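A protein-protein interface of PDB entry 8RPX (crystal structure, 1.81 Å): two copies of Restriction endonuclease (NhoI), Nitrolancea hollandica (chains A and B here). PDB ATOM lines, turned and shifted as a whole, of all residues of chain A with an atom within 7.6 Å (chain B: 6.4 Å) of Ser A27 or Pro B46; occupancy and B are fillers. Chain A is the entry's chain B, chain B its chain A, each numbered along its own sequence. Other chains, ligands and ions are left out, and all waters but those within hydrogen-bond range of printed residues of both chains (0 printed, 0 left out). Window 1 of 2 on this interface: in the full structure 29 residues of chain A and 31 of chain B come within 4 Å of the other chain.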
ATOM      1  N   ARG A  21      -2.048   1.906 -22.983  1.00  0.00           N
ATOM      2  CA  ARG A  21      -1.329   2.520 -24.098  1.00  0.00           C
ATOM      3  C   ARG A  21      -1.202   4.029 -23.891  1.00  0.00           C
ATOM      4  O   ARG A  21      -0.100   4.587 -23.986  1.00  0.00           O
ATOM      5  CB  ARG A  21      -2.026   2.172 -25.415  1.00  0.00           C
ATOM      6  CG  ARG A  21      -1.384   2.740 -26.669  1.00  0.00           C
ATOM      7  CD  ARG A  21      -2.082   2.224 -27.933  1.00  0.00           C
ATOM      8  NE  ARG A  21      -1.381   2.623 -29.149  1.00  0.00           N
ATOM      9  CZ  ARG A  21      -1.596   2.109 -30.355  1.00  0.00           C
ATOM     10  NH1 ARG A  21      -2.474   1.134 -30.550  1.00  0.00           N
ATOM     11  NH2 ARG A  21      -0.930   2.600 -31.398  1.00  0.00           N
ATOM     12  N   GLU A  22      -2.304   4.688 -23.503  1.00  0.00           N
ATOM     13  CA  GLU A  22      -2.257   6.121 -23.217  1.00  0.00           C
ATOM     14  C   GLU A  22      -1.355   6.445 -22.033  1.00  0.00           C
ATOM     15  O   GLU A  22      -0.657   7.467 -22.038  1.00  0.00           O
ATOM     16  CB  GLU A  22      -3.662   6.646 -22.920  1.00  0.00           C
ATOM     17  CG  GLU A  22      -4.565   6.802 -24.107  1.00  0.00           C
ATOM     18  CD  GLU A  22      -5.987   7.161 -23.699  1.00  0.00           C
ATOM     19  OE1 GLU A  22      -6.555   6.482 -22.816  1.00  0.00           O
ATOM     20  OE2 GLU A  22      -6.525   8.137 -24.255  1.00  0.00           O
ATOM     21  N   LEU A  23      -1.364   5.601 -21.001  1.00  0.00           N
ATOM     22  CA  LEU A  23      -0.503   5.833 -19.847  1.00  0.00           C
ATOM     23  C   LEU A  23       0.962   5.829 -20.251  1.00  0.00           C
ATOM     24  O   LEU A  23       1.743   6.690 -19.830  1.00  0.00           O
ATOM     25  CB  LEU A  23      -0.750   4.766 -18.790  1.00  0.00           C
ATOM     26  CG  LEU A  23      -1.809   5.048 -17.741  1.00  0.00           C
ATOM     27  CD1 LEU A  23      -1.871   3.832 -16.848  1.00  0.00           C
ATOM     28  CD2 LEU A  23      -1.442   6.300 -16.976  1.00  0.00           C
ATOM     29  N   LEU A  24       1.353   4.844 -21.059  1.00  0.00           N
ATOM     30  CA  LEU A  24       2.729   4.776 -21.537  1.00  0.00           C
ATOM     31  C   LEU A  24       3.059   5.972 -22.423  1.00  0.00           C
ATOM     32  O   LEU A  24       4.167   6.513 -22.362  1.00  0.00           O
ATOM     33  CB  LEU A  24       2.937   3.459 -22.281  1.00  0.00           C
ATOM     34  CG  LEU A  24       2.820   2.263 -21.334  1.00  0.00           C
ATOM     35  CD1 LEU A  24       2.639   0.964 -22.095  1.00  0.00           C
ATOM     36  CD2 LEU A  24       4.055   2.226 -20.405  1.00  0.00           C
ATOM     37  N   ALA A  25       2.101   6.409 -23.246  1.00  0.00           N
ATOM     38  CA  ALA A  25       2.342   7.567 -24.098  1.00  0.00           C
ATOM     39  C   ALA A  25       2.495   8.834 -23.270  1.00  0.00           C
ATOM     40  O   ALA A  25       3.334   9.684 -23.579  1.00  0.00           O
ATOM     41  CB  ALA A  25       1.213   7.720 -25.119  1.00  0.00           C
ATOM     42  N   VAL A  26       1.709   8.969 -22.204  1.00  0.00           N
ATOM     43  CA  VAL A  26       1.843  10.136 -21.342  1.00  0.00           C
ATOM     44  C   VAL A  26       3.201  10.127 -20.657  1.00  0.00           C
ATOM     45  O   VAL A  26       3.815  11.179 -20.440  1.00  0.00           O
ATOM     46  CB  VAL A  26       0.698  10.174 -20.314  1.00  0.00           C
ATOM     47  CG1 VAL A  26       0.972  11.217 -19.240  1.00  0.00           C
ATOM     48  CG2 VAL A  26      -0.610  10.452 -20.996  1.00  0.00           C
ATOM     49  N   SER A  27       3.692   8.943 -20.302  1.00  0.00           N
ATOM     50  CA  SER A  27       5.019   8.848 -19.703  1.00  0.00           C
ATOM     51  C   SER A  27       6.084   9.422 -20.635  1.00  0.00           C
ATOM     52  O   SER A  27       6.934  10.214 -20.207  1.00  0.00           O
ATOM     53  CB  SER A  27       5.315   7.392 -19.334  1.00  0.00           C
ATOM     54  OG  SER A  27       6.644   7.223 -18.886  1.00  0.00           O
ATOM     55  N   ARG A  28       6.031   9.056 -21.929  1.00  0.00           N
ATOM     56  CA  ARG A  28       6.998   9.564 -22.903  1.00  0.00           C
ATOM     57  C   ARG A  28       6.774  11.036 -23.212  1.00  0.00           C
ATOM     58  O   ARG A  28       7.736  11.804 -23.302  1.00  0.00           O
ATOM     59  CB  ARG A  28       6.929   8.765 -24.210  1.00  0.00           C
ATOM     60  CG  ARG A  28       7.166   7.283 -24.089  1.00  0.00           C
ATOM     61  CD  ARG A  28       8.479   6.990 -23.384  1.00  0.00           C
ATOM     62  NE  ARG A  28       9.653   7.472 -24.100  1.00  0.00           N
ATOM     63  CZ  ARG A  28      10.884   7.411 -23.602  1.00  0.00           C
ATOM     64  NH1 ARG A  28      11.117   6.923 -22.394  1.00  0.00           N
ATOM     65  NH2 ARG A  28      11.904   7.847 -24.337  1.00  0.00           N
ATOM     66  N   ALA A  29       5.517  11.444 -23.420  1.00  0.00           N
ATOM     67  CA  ALA A  29       5.243  12.826 -23.812  1.00  0.00           C
ATOM     68  C   ALA A  29       5.650  13.806 -22.715  1.00  0.00           C
ATOM     69  O   ALA A  29       6.150  14.898 -23.005  1.00  0.00           O
ATOM     70  CB  ALA A  29       3.764  12.993 -24.173  1.00  0.00           C
ATOM     71  N   SER A  30       5.429  13.441 -21.449  1.00  0.00           N
ATOM     72  CA  SER A  30       5.821  14.329 -20.356  1.00  0.00           C
ATOM     73  C   SER A  30       7.334  14.489 -20.306  1.00  0.00           C
ATOM     74  O   SER A  30       7.845  15.597 -20.099  1.00  0.00           O
ATOM     75  CB  SER A  30       5.280  13.801 -19.028  1.00  0.00           C
ATOM     76  OG  SER A  30       5.871  12.563 -18.691  1.00  0.00           O
ATOM     77  N   LEU A  31       8.060  13.394 -20.532  1.00  0.00           N
ATOM     78  CA  LEU A  31       9.509  13.473 -20.678  1.00  0.00           C
ATOM     79  C   LEU A  31       9.889  14.396 -21.837  1.00  0.00           C
ATOM     80  O   LEU A  31      10.758  15.265 -21.690  1.00  0.00           O
ATOM     81  CB  LEU A  31      10.062  12.064 -20.884  1.00  0.00           C
ATOM     82  CG  LEU A  31      11.509  11.700 -20.587  1.00  0.00           C
ATOM     83  CD1 LEU A  31      11.815  11.784 -19.116  1.00  0.00           C
ATOM     84  CD2 LEU A  31      11.741  10.290 -21.085  1.00  0.00           C
ATOM     85  N   ARG A  32       9.226  14.238 -22.995  1.00  0.00           N
ATOM     86  CA  ARG A  32       9.546  15.071 -24.154  1.00  0.00           C
ATOM     87  C   ARG A  32       9.277  16.543 -23.873  1.00  0.00           C
ATOM     88  O   ARG A  32      10.057  17.411 -24.279  1.00  0.00           O
ATOM     89  CB  ARG A  32       8.757  14.618 -25.390  1.00  0.00           C
ATOM     90  CG  ARG A  32       9.388  13.458 -26.145  1.00  0.00           C
ATOM     91  CD  ARG A  32       8.802  13.278 -27.551  1.00  0.00           C
ATOM     92  NE  ARG A  32       7.359  13.074 -27.557  1.00  0.00           N
ATOM     93  CZ  ARG A  32       6.770  11.897 -27.390  1.00  0.00           C
ATOM     94  NH1 ARG A  32       7.472  10.795 -27.177  1.00  0.00           N
ATOM     95  NH2 ARG A  32       5.442  11.824 -27.437  1.00  0.00           N
ATOM     96  N   GLU A  33       8.173  16.850 -23.189  1.00  0.00           N
ATOM     97  CA  GLU A  33       7.866  18.246 -22.894  1.00  0.00           C
ATOM     98  C   GLU A  33       8.834  18.822 -21.864  1.00  0.00           C
ATOM     99  O   GLU A  33       9.250  19.983 -21.974  1.00  0.00           O
ATOM    100  CB  GLU A  33       6.430  18.376 -22.389  1.00  0.00           C
ATOM    101  CG  GLU A  33       6.069  19.794 -22.014  1.00  0.00           C
ATOM    102  CD  GLU A  33       6.130  20.746 -23.189  1.00  0.00           C
ATOM    103  OE1 GLU A  33       6.041  20.286 -24.350  1.00  0.00           O
ATOM    104  OE2 GLU A  33       6.296  21.960 -22.947  1.00  0.00           O
ATOM    105  N   LEU A  34       9.215  18.024 -20.868  1.00  0.00           N
ATOM    106  CA  LEU A  34      10.201  18.498 -19.906  1.00  0.00           C
ATOM    107  C   LEU A  34      11.523  18.802 -20.594  1.00  0.00           C
ATOM    108  O   LEU A  34      12.162  19.821 -20.306  1.00  0.00           O
ATOM    109  CB  LEU A  34      10.389  17.472 -18.789  1.00  0.00           C
ATOM    110  CG  LEU A  34       9.243  17.393 -17.779  1.00  0.00           C
ATOM    111  CD1 LEU A  34       9.355  16.145 -16.908  1.00  0.00           C
ATOM    112  CD2 LEU A  34       9.219  18.656 -16.923  1.00  0.00           C
ATOM    113  N   ALA A  45      14.817   8.778 -16.488  1.00  0.00           N
ATOM    114  CA  ALA A  45      13.715   9.317 -15.694  1.00  0.00           C
ATOM    115  C   ALA A  45      14.140  10.693 -15.168  1.00  0.00           C
ATOM    116  O   ALA A  45      15.335  10.930 -14.909  1.00  0.00           O
ATOM    117  CB  ALA A  45      13.335   8.377 -14.536  1.00  0.00           C
ATOM    118  N   PRO A  46      13.201  11.627 -15.020  1.00  0.00           N
ATOM    119  CA  PRO A  46      13.582  13.038 -14.844  1.00  0.00           C
ATOM    120  C   PRO A  46      14.307  13.376 -13.552  1.00  0.00           C
ATOM    121  O   PRO A  46      14.888  14.466 -13.487  1.00  0.00           O
ATOM    122  CB  PRO A  46      12.239  13.781 -14.910  1.00  0.00           C
ATOM    123  CG  PRO A  46      11.180  12.728 -14.730  1.00  0.00           C
ATOM    124  CD  PRO A  46      11.755  11.458 -15.256  1.00  0.00           C
ATOM    125  N   SER B  27       4.251  13.138 -14.312  1.00  0.00           N
ATOM    126  CA  SER B  27       5.282  12.112 -14.436  1.00  0.00           C
ATOM    127  C   SER B  27       5.177  11.086 -13.308  1.00  0.00           C
ATOM    128  O   SER B  27       5.268   9.878 -13.546  1.00  0.00           O
ATOM    129  CB  SER B  27       6.668  12.764 -14.443  1.00  0.00           C
ATOM    130  OG  SER B  27       7.698  11.796 -14.404  1.00  0.00           O
ATOM    131  N   SER B  30       1.533   9.084 -13.490  1.00  0.00           N
ATOM    132  CA  SER B  30       1.435   8.018 -14.483  1.00  0.00           C
ATOM    133  C   SER B  30       2.213   6.785 -14.037  1.00  0.00           C
ATOM    134  O   SER B  30       1.751   5.651 -14.213  1.00  0.00           O
ATOM    135  CB  SER B  30       1.903   8.517 -15.855  1.00  0.00           C
ATOM    136  OG  SER B  30       3.288   8.813 -15.894  1.00  0.00           O
ATOM    137  N   LEU B  31       3.384   6.988 -13.435  1.00  0.00           N
ATOM    138  CA  LEU B  31       4.122   5.874 -12.852  1.00  0.00           C
ATOM    139  C   LEU B  31       3.291   5.155 -11.788  1.00  0.00           C
ATOM    140  O   LEU B  31       3.214   3.922 -11.777  1.00  0.00           O
ATOM    141  CB  LEU B  31       5.431   6.385 -12.267  1.00  0.00           C
ATOM    142  CG  LEU B  31       6.565   5.383 -12.089  1.00  0.00           C
ATOM    143  CD1 LEU B  31       7.064   4.909 -13.445  1.00  0.00           C
ATOM    144  CD2 LEU B  31       7.678   6.036 -11.279  1.00  0.00           C
ATOM    145  N   LEU B  34       0.488   3.097 -13.469  1.00  0.00           N
ATOM    146  CA  LEU B  34       1.014   1.898 -14.107  1.00  0.00           C
ATOM    147  C   LEU B  34       1.321   0.812 -13.081  1.00  0.00           C
ATOM    148  O   LEU B  34       1.019  -0.364 -13.312  1.00  0.00           O
ATOM    149  CB  LEU B  34       2.256   2.238 -14.929  1.00  0.00           C
ATOM    150  CG  LEU B  34       1.970   2.975 -16.241  1.00  0.00           C
ATOM    151  CD1 LEU B  34       3.255   3.560 -16.790  1.00  0.00           C
ATOM    152  CD2 LEU B  34       1.368   2.014 -17.238  1.00  0.00           C
ATOM    153  N   VAL B  39       1.191  -3.084 -14.474  1.00  0.00           N
ATOM    154  CA  VAL B  39       1.966  -3.023 -15.709  1.00  0.00           C
ATOM    155  C   VAL B  39       3.450  -2.990 -15.390  1.00  0.00           C
ATOM    156  O   VAL B  39       4.266  -3.609 -16.080  1.00  0.00           O
ATOM    157  CB  VAL B  39       1.538  -1.808 -16.552  1.00  0.00           C
ATOM    158  CG1 VAL B  39       2.422  -1.681 -17.789  1.00  0.00           C
ATOM    159  CG2 VAL B  39       0.064  -1.948 -16.950  1.00  0.00           C
ATOM    160  N   ILE B  40       3.815  -2.284 -14.323  1.00  0.00           N
ATOM    161  CA  ILE B  40       5.168  -2.252 -13.802  1.00  0.00           C
ATOM    162  C   ILE B  40       5.081  -2.650 -12.334  1.00  0.00           C
ATOM    163  O   ILE B  40       3.996  -2.752 -11.763  1.00  0.00           O
ATOM    164  CB  ILE B  40       5.820  -0.870 -13.951  1.00  0.00           C
ATOM    165  CG1 ILE B  40       5.049   0.166 -13.133  1.00  0.00           C
ATOM    166  CG2 ILE B  40       5.919  -0.476 -15.445  1.00  0.00           C
ATOM    167  CD1 ILE B  40       5.646   1.561 -13.242  1.00  0.00           C
ATOM    168  N   ASN B  44      11.280   2.345 -11.163  1.00  0.00           N
ATOM    169  CA  ASN B  44      12.105   2.657 -12.325  1.00  0.00           C
ATOM    170  C   ASN B  44      11.251   3.254 -13.443  1.00  0.00           C
ATOM    171  O   ASN B  44      10.022   3.150 -13.445  1.00  0.00           O
ATOM    172  CB  ASN B  44      12.803   1.396 -12.845  1.00  0.00           C
ATOM    173  CG  ASN B  44      13.822   0.819 -11.856  1.00  0.00           C
ATOM    174  OD1 ASN B  44      14.562   1.546 -11.189  1.00  0.00           O
ATOM    175  ND2 ASN B  44      13.874  -0.510 -11.783  1.00  0.00           N
ATOM    176  N   ALA B  45      11.921   3.877 -14.422  1.00  0.00           N
ATOM    177  CA  ALA B  45      11.210   4.235 -15.647  1.00  0.00           C
ATOM    178  C   ALA B  45      10.553   2.972 -16.192  1.00  0.00           C
ATOM    179  O   ALA B  45      11.096   1.870 -16.031  1.00  0.00           O
ATOM    180  CB  ALA B  45      12.152   4.857 -16.683  1.00  0.00           C
ATOM    181  N   PRO B  46       9.374   3.090 -16.804  1.00  0.00           N
ATOM    182  CA  PRO B  46       8.563   1.894 -17.084  1.00  0.00           C
ATOM    183  C   PRO B  46       9.176   0.899 -18.059  1.00  0.00           C
ATOM    184  O   PRO B  46       8.738  -0.262 -18.059  1.00  0.00           O
ATOM    185  CB  PRO B  46       7.265   2.476 -17.658  1.00  0.00           C
ATOM    186  CG  PRO B  46       7.238   3.883 -17.211  1.00  0.00           C
ATOM    187  CD  PRO B  46       8.655   4.335 -17.113  1.00  0.00           C
ATOM    188  N   ALA B  47      10.172   1.292 -18.868  1.00  0.00           N
ATOM    189  CA  ALA B  47      10.584   0.445 -19.986  1.00  0.00           C
ATOM    190  C   ALA B  47      11.019  -0.935 -19.520  1.00  0.00           C
ATOM    191  O   ALA B  47      10.637  -1.949 -20.121  1.00  0.00           O
ATOM    192  CB  ALA B  47      11.705   1.113 -20.791  1.00  0.00           C
ATOM    193  N   GLY B  48      11.834  -0.993 -18.459  1.00  0.00           N
ATOM    194  CA  GLY B  48      12.351  -2.275 -18.007  1.00  0.00           C
ATOM    195  C   GLY B  48      11.261  -3.247 -17.571  1.00  0.00           C
ATOM    196  O   GLY B  48      11.220  -4.397 -18.021  1.00  0.00           O
ATOM    197  N   ASP B  49      10.378  -2.811 -16.665  1.00  0.00           N
ATOM    198  CA  ASP B  49       9.321  -3.706 -16.186  1.00  0.00           C
ATOM    199  C   ASP B  49       8.312  -4.018 -17.289  1.00  0.00           C
ATOM    200  O   ASP B  49       7.798  -5.143 -17.375  1.00  0.00           O
ATOM    201  CB  ASP B  49       8.586  -3.101 -14.979  1.00  0.00           C
ATOM    202  CG  ASP B  49       9.372  -3.207 -13.681  1.00  0.00           C
ATOM    203  OD1 ASP B  49      10.395  -3.934 -13.639  1.00  0.00           O
ATOM    204  OD2 ASP B  49       8.934  -2.574 -12.676  1.00  0.00           O
ATOM    205  N   TYR B  50       8.004  -3.037 -18.128  1.00  0.00           N
ATOM    206  CA  TYR B  50       7.009  -3.258 -19.168  1.00  0.00           C
ATOM    207  C   TYR B  50       7.499  -4.276 -20.200  1.00  0.00           C
ATOM    208  O   TYR B  50       6.740  -5.158 -20.611  1.00  0.00           O
ATOM    209  CB  TYR B  50       6.642  -1.928 -19.823  1.00  0.00           C
ATOM    210  CG  TYR B  50       5.591  -2.068 -20.901  1.00  0.00           C
ATOM    211  CD1 TYR B  50       4.401  -2.724 -20.658  1.00  0.00           C
ATOM    212  CD2 TYR B  50       5.807  -1.543 -22.175  1.00  0.00           C
ATOM    213  CE1 TYR B  50       3.449  -2.850 -21.651  1.00  0.00           C
ATOM    214  CE2 TYR B  50       4.868  -1.669 -23.174  1.00  0.00           C
ATOM    215  CZ  TYR B  50       3.702  -2.323 -22.920  1.00  0.00           C
ATOM    216  OH  TYR B  50       2.769  -2.437 -23.923  1.00  0.00           O
ATOM    217  N   ALA B  51       8.774  -4.198 -20.589  1.00  0.00           N
ATOM    218  CA  ALA B  51       9.340  -5.210 -21.478  1.00  0.00           C
ATOM    219  C   ALA B  51       9.293  -6.601 -20.848  1.00  0.00           C
ATOM    220  O   ALA B  51       8.992  -7.583 -21.532  1.00  0.00           O
ATOM    221  CB  ALA B  51      10.778  -4.840 -21.853  1.00  0.00           C
ATOM    222  N   PHE B 115      11.650  -0.560 -28.129  1.00  0.00           N
ATOM    223  CA  PHE B 115      10.427   0.227 -28.227  1.00  0.00           C
ATOM    224  C   PHE B 115      10.655   1.437 -29.113  1.00  0.00           C
ATOM    225  O   PHE B 115      11.778   1.936 -29.214  1.00  0.00           O
ATOM    226  CB  PHE B 115       9.971   0.732 -26.858  1.00  0.00           C
ATOM    227  CG  PHE B 115       9.566  -0.349 -25.909  1.00  0.00           C
ATOM    228  CD1 PHE B 115       8.385  -1.068 -26.118  1.00  0.00           C
ATOM    229  CD2 PHE B 115      10.320  -0.608 -24.776  1.00  0.00           C
ATOM    230  CE1 PHE B 115       7.993  -2.066 -25.210  1.00  0.00           C
ATOM    231  CE2 PHE B 115       9.931  -1.595 -23.852  1.00  0.00           C
ATOM    232  CZ  PHE B 115       8.770  -2.325 -24.085  1.00  0.00           C
ATOM    233  N   PHE B 119       6.299   4.082 -27.034  1.00  0.00           N
ATOM    234  CA  PHE B 119       6.272   2.857 -26.237  1.00  0.00           C
ATOM    235  C   PHE B 119       5.591   1.687 -26.937  1.00  0.00           C
ATOM    236  O   PHE B 119       5.107   0.765 -26.270  1.00  0.00           O
ATOM    237  CB  PHE B 119       5.638   3.075 -24.851  1.00  0.00           C
ATOM    238  CG  PHE B 119       6.618   3.004 -23.739  1.00  0.00           C
ATOM    239  CD1 PHE B 119       7.368   1.857 -23.564  1.00  0.00           C
ATOM    240  CD2 PHE B 119       6.806   4.073 -22.868  1.00  0.00           C
ATOM    241  CE1 PHE B 119       8.304   1.776 -22.555  1.00  0.00           C
ATOM    242  CE2 PHE B 119       7.726   3.999 -21.853  1.00  0.00           C
ATOM    243  CZ  PHE B 119       8.482   2.851 -21.690  1.00  0.00           C
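N of Val B39 lies within hydrogen-bond range of O of Leu B34, at 3.0 Å. The side-chain hydroxyl of Ser A30 is in hydrogen-bond range of the backbone carbonyl oxygen of Ser A27, 3.0 Å away. OG of Ser B30 sits at hydrogen-bond distance from O of Ser B27 (3.3 Å).
Ser A27 touches Pro B46, and with the chains exchanged Pro A46 touches Ser B27. Of the 7 pairs that touch across the chains among the printed residues, 2 have their exchanged pair printed and touching as well.
Of the 16 printed residues of chain A, 5 touch a printed residue of chain B. Hydrophobic or aromatic side chains of chain A that line the printed part of chain B: Leu A23, Leu A24 and Pro A46. Among the printed residues, 7 pairs touch across the chains. Among the printed residues, no Asp or Glu carboxylate lies within 4 Å of a Lys or Arg side-chain nitrogen of the other chain.
Ser A27 touches just one residue of chain B: Pro B46 (3.8 Å). Pro B46 touches just one residue of chain A: Ser A27. Printed residues of chain B within 4 Å of Pro A46: Ser B27 (3.6 Å). Printed residues of chain A within 4 Å of Phe B119: Leu A24 (3.6 Å) and Arg A28 (3.4 Å). Of the printed residues of chain B, Leu A24 touches Leu B34, Tyr B50 and Phe B119. Glu A33 touches none of the printed residues of chain B. Asn B44 touches none of the printed residues of chain A. The nearest residue of chain A that does not touch Pro B46 is Leu A24 (4.2 Å).
Leu B34 touches Leu A23 (CD2 to CD1, 3.7 Å). Leu B34 touches Leu A24 (CD1 to CD2, 3.9 Å). Tyr B50 touches Leu A24. Leu A24 touches Phe B119 (O to CD2, 3.6 Å). CG of Pro B46 touches OG of Ser A27, at 3.8 Å. Arg A28 touches Phe B119. OG of Ser B27 touches CG of Pro A46, 3.6 Å away.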
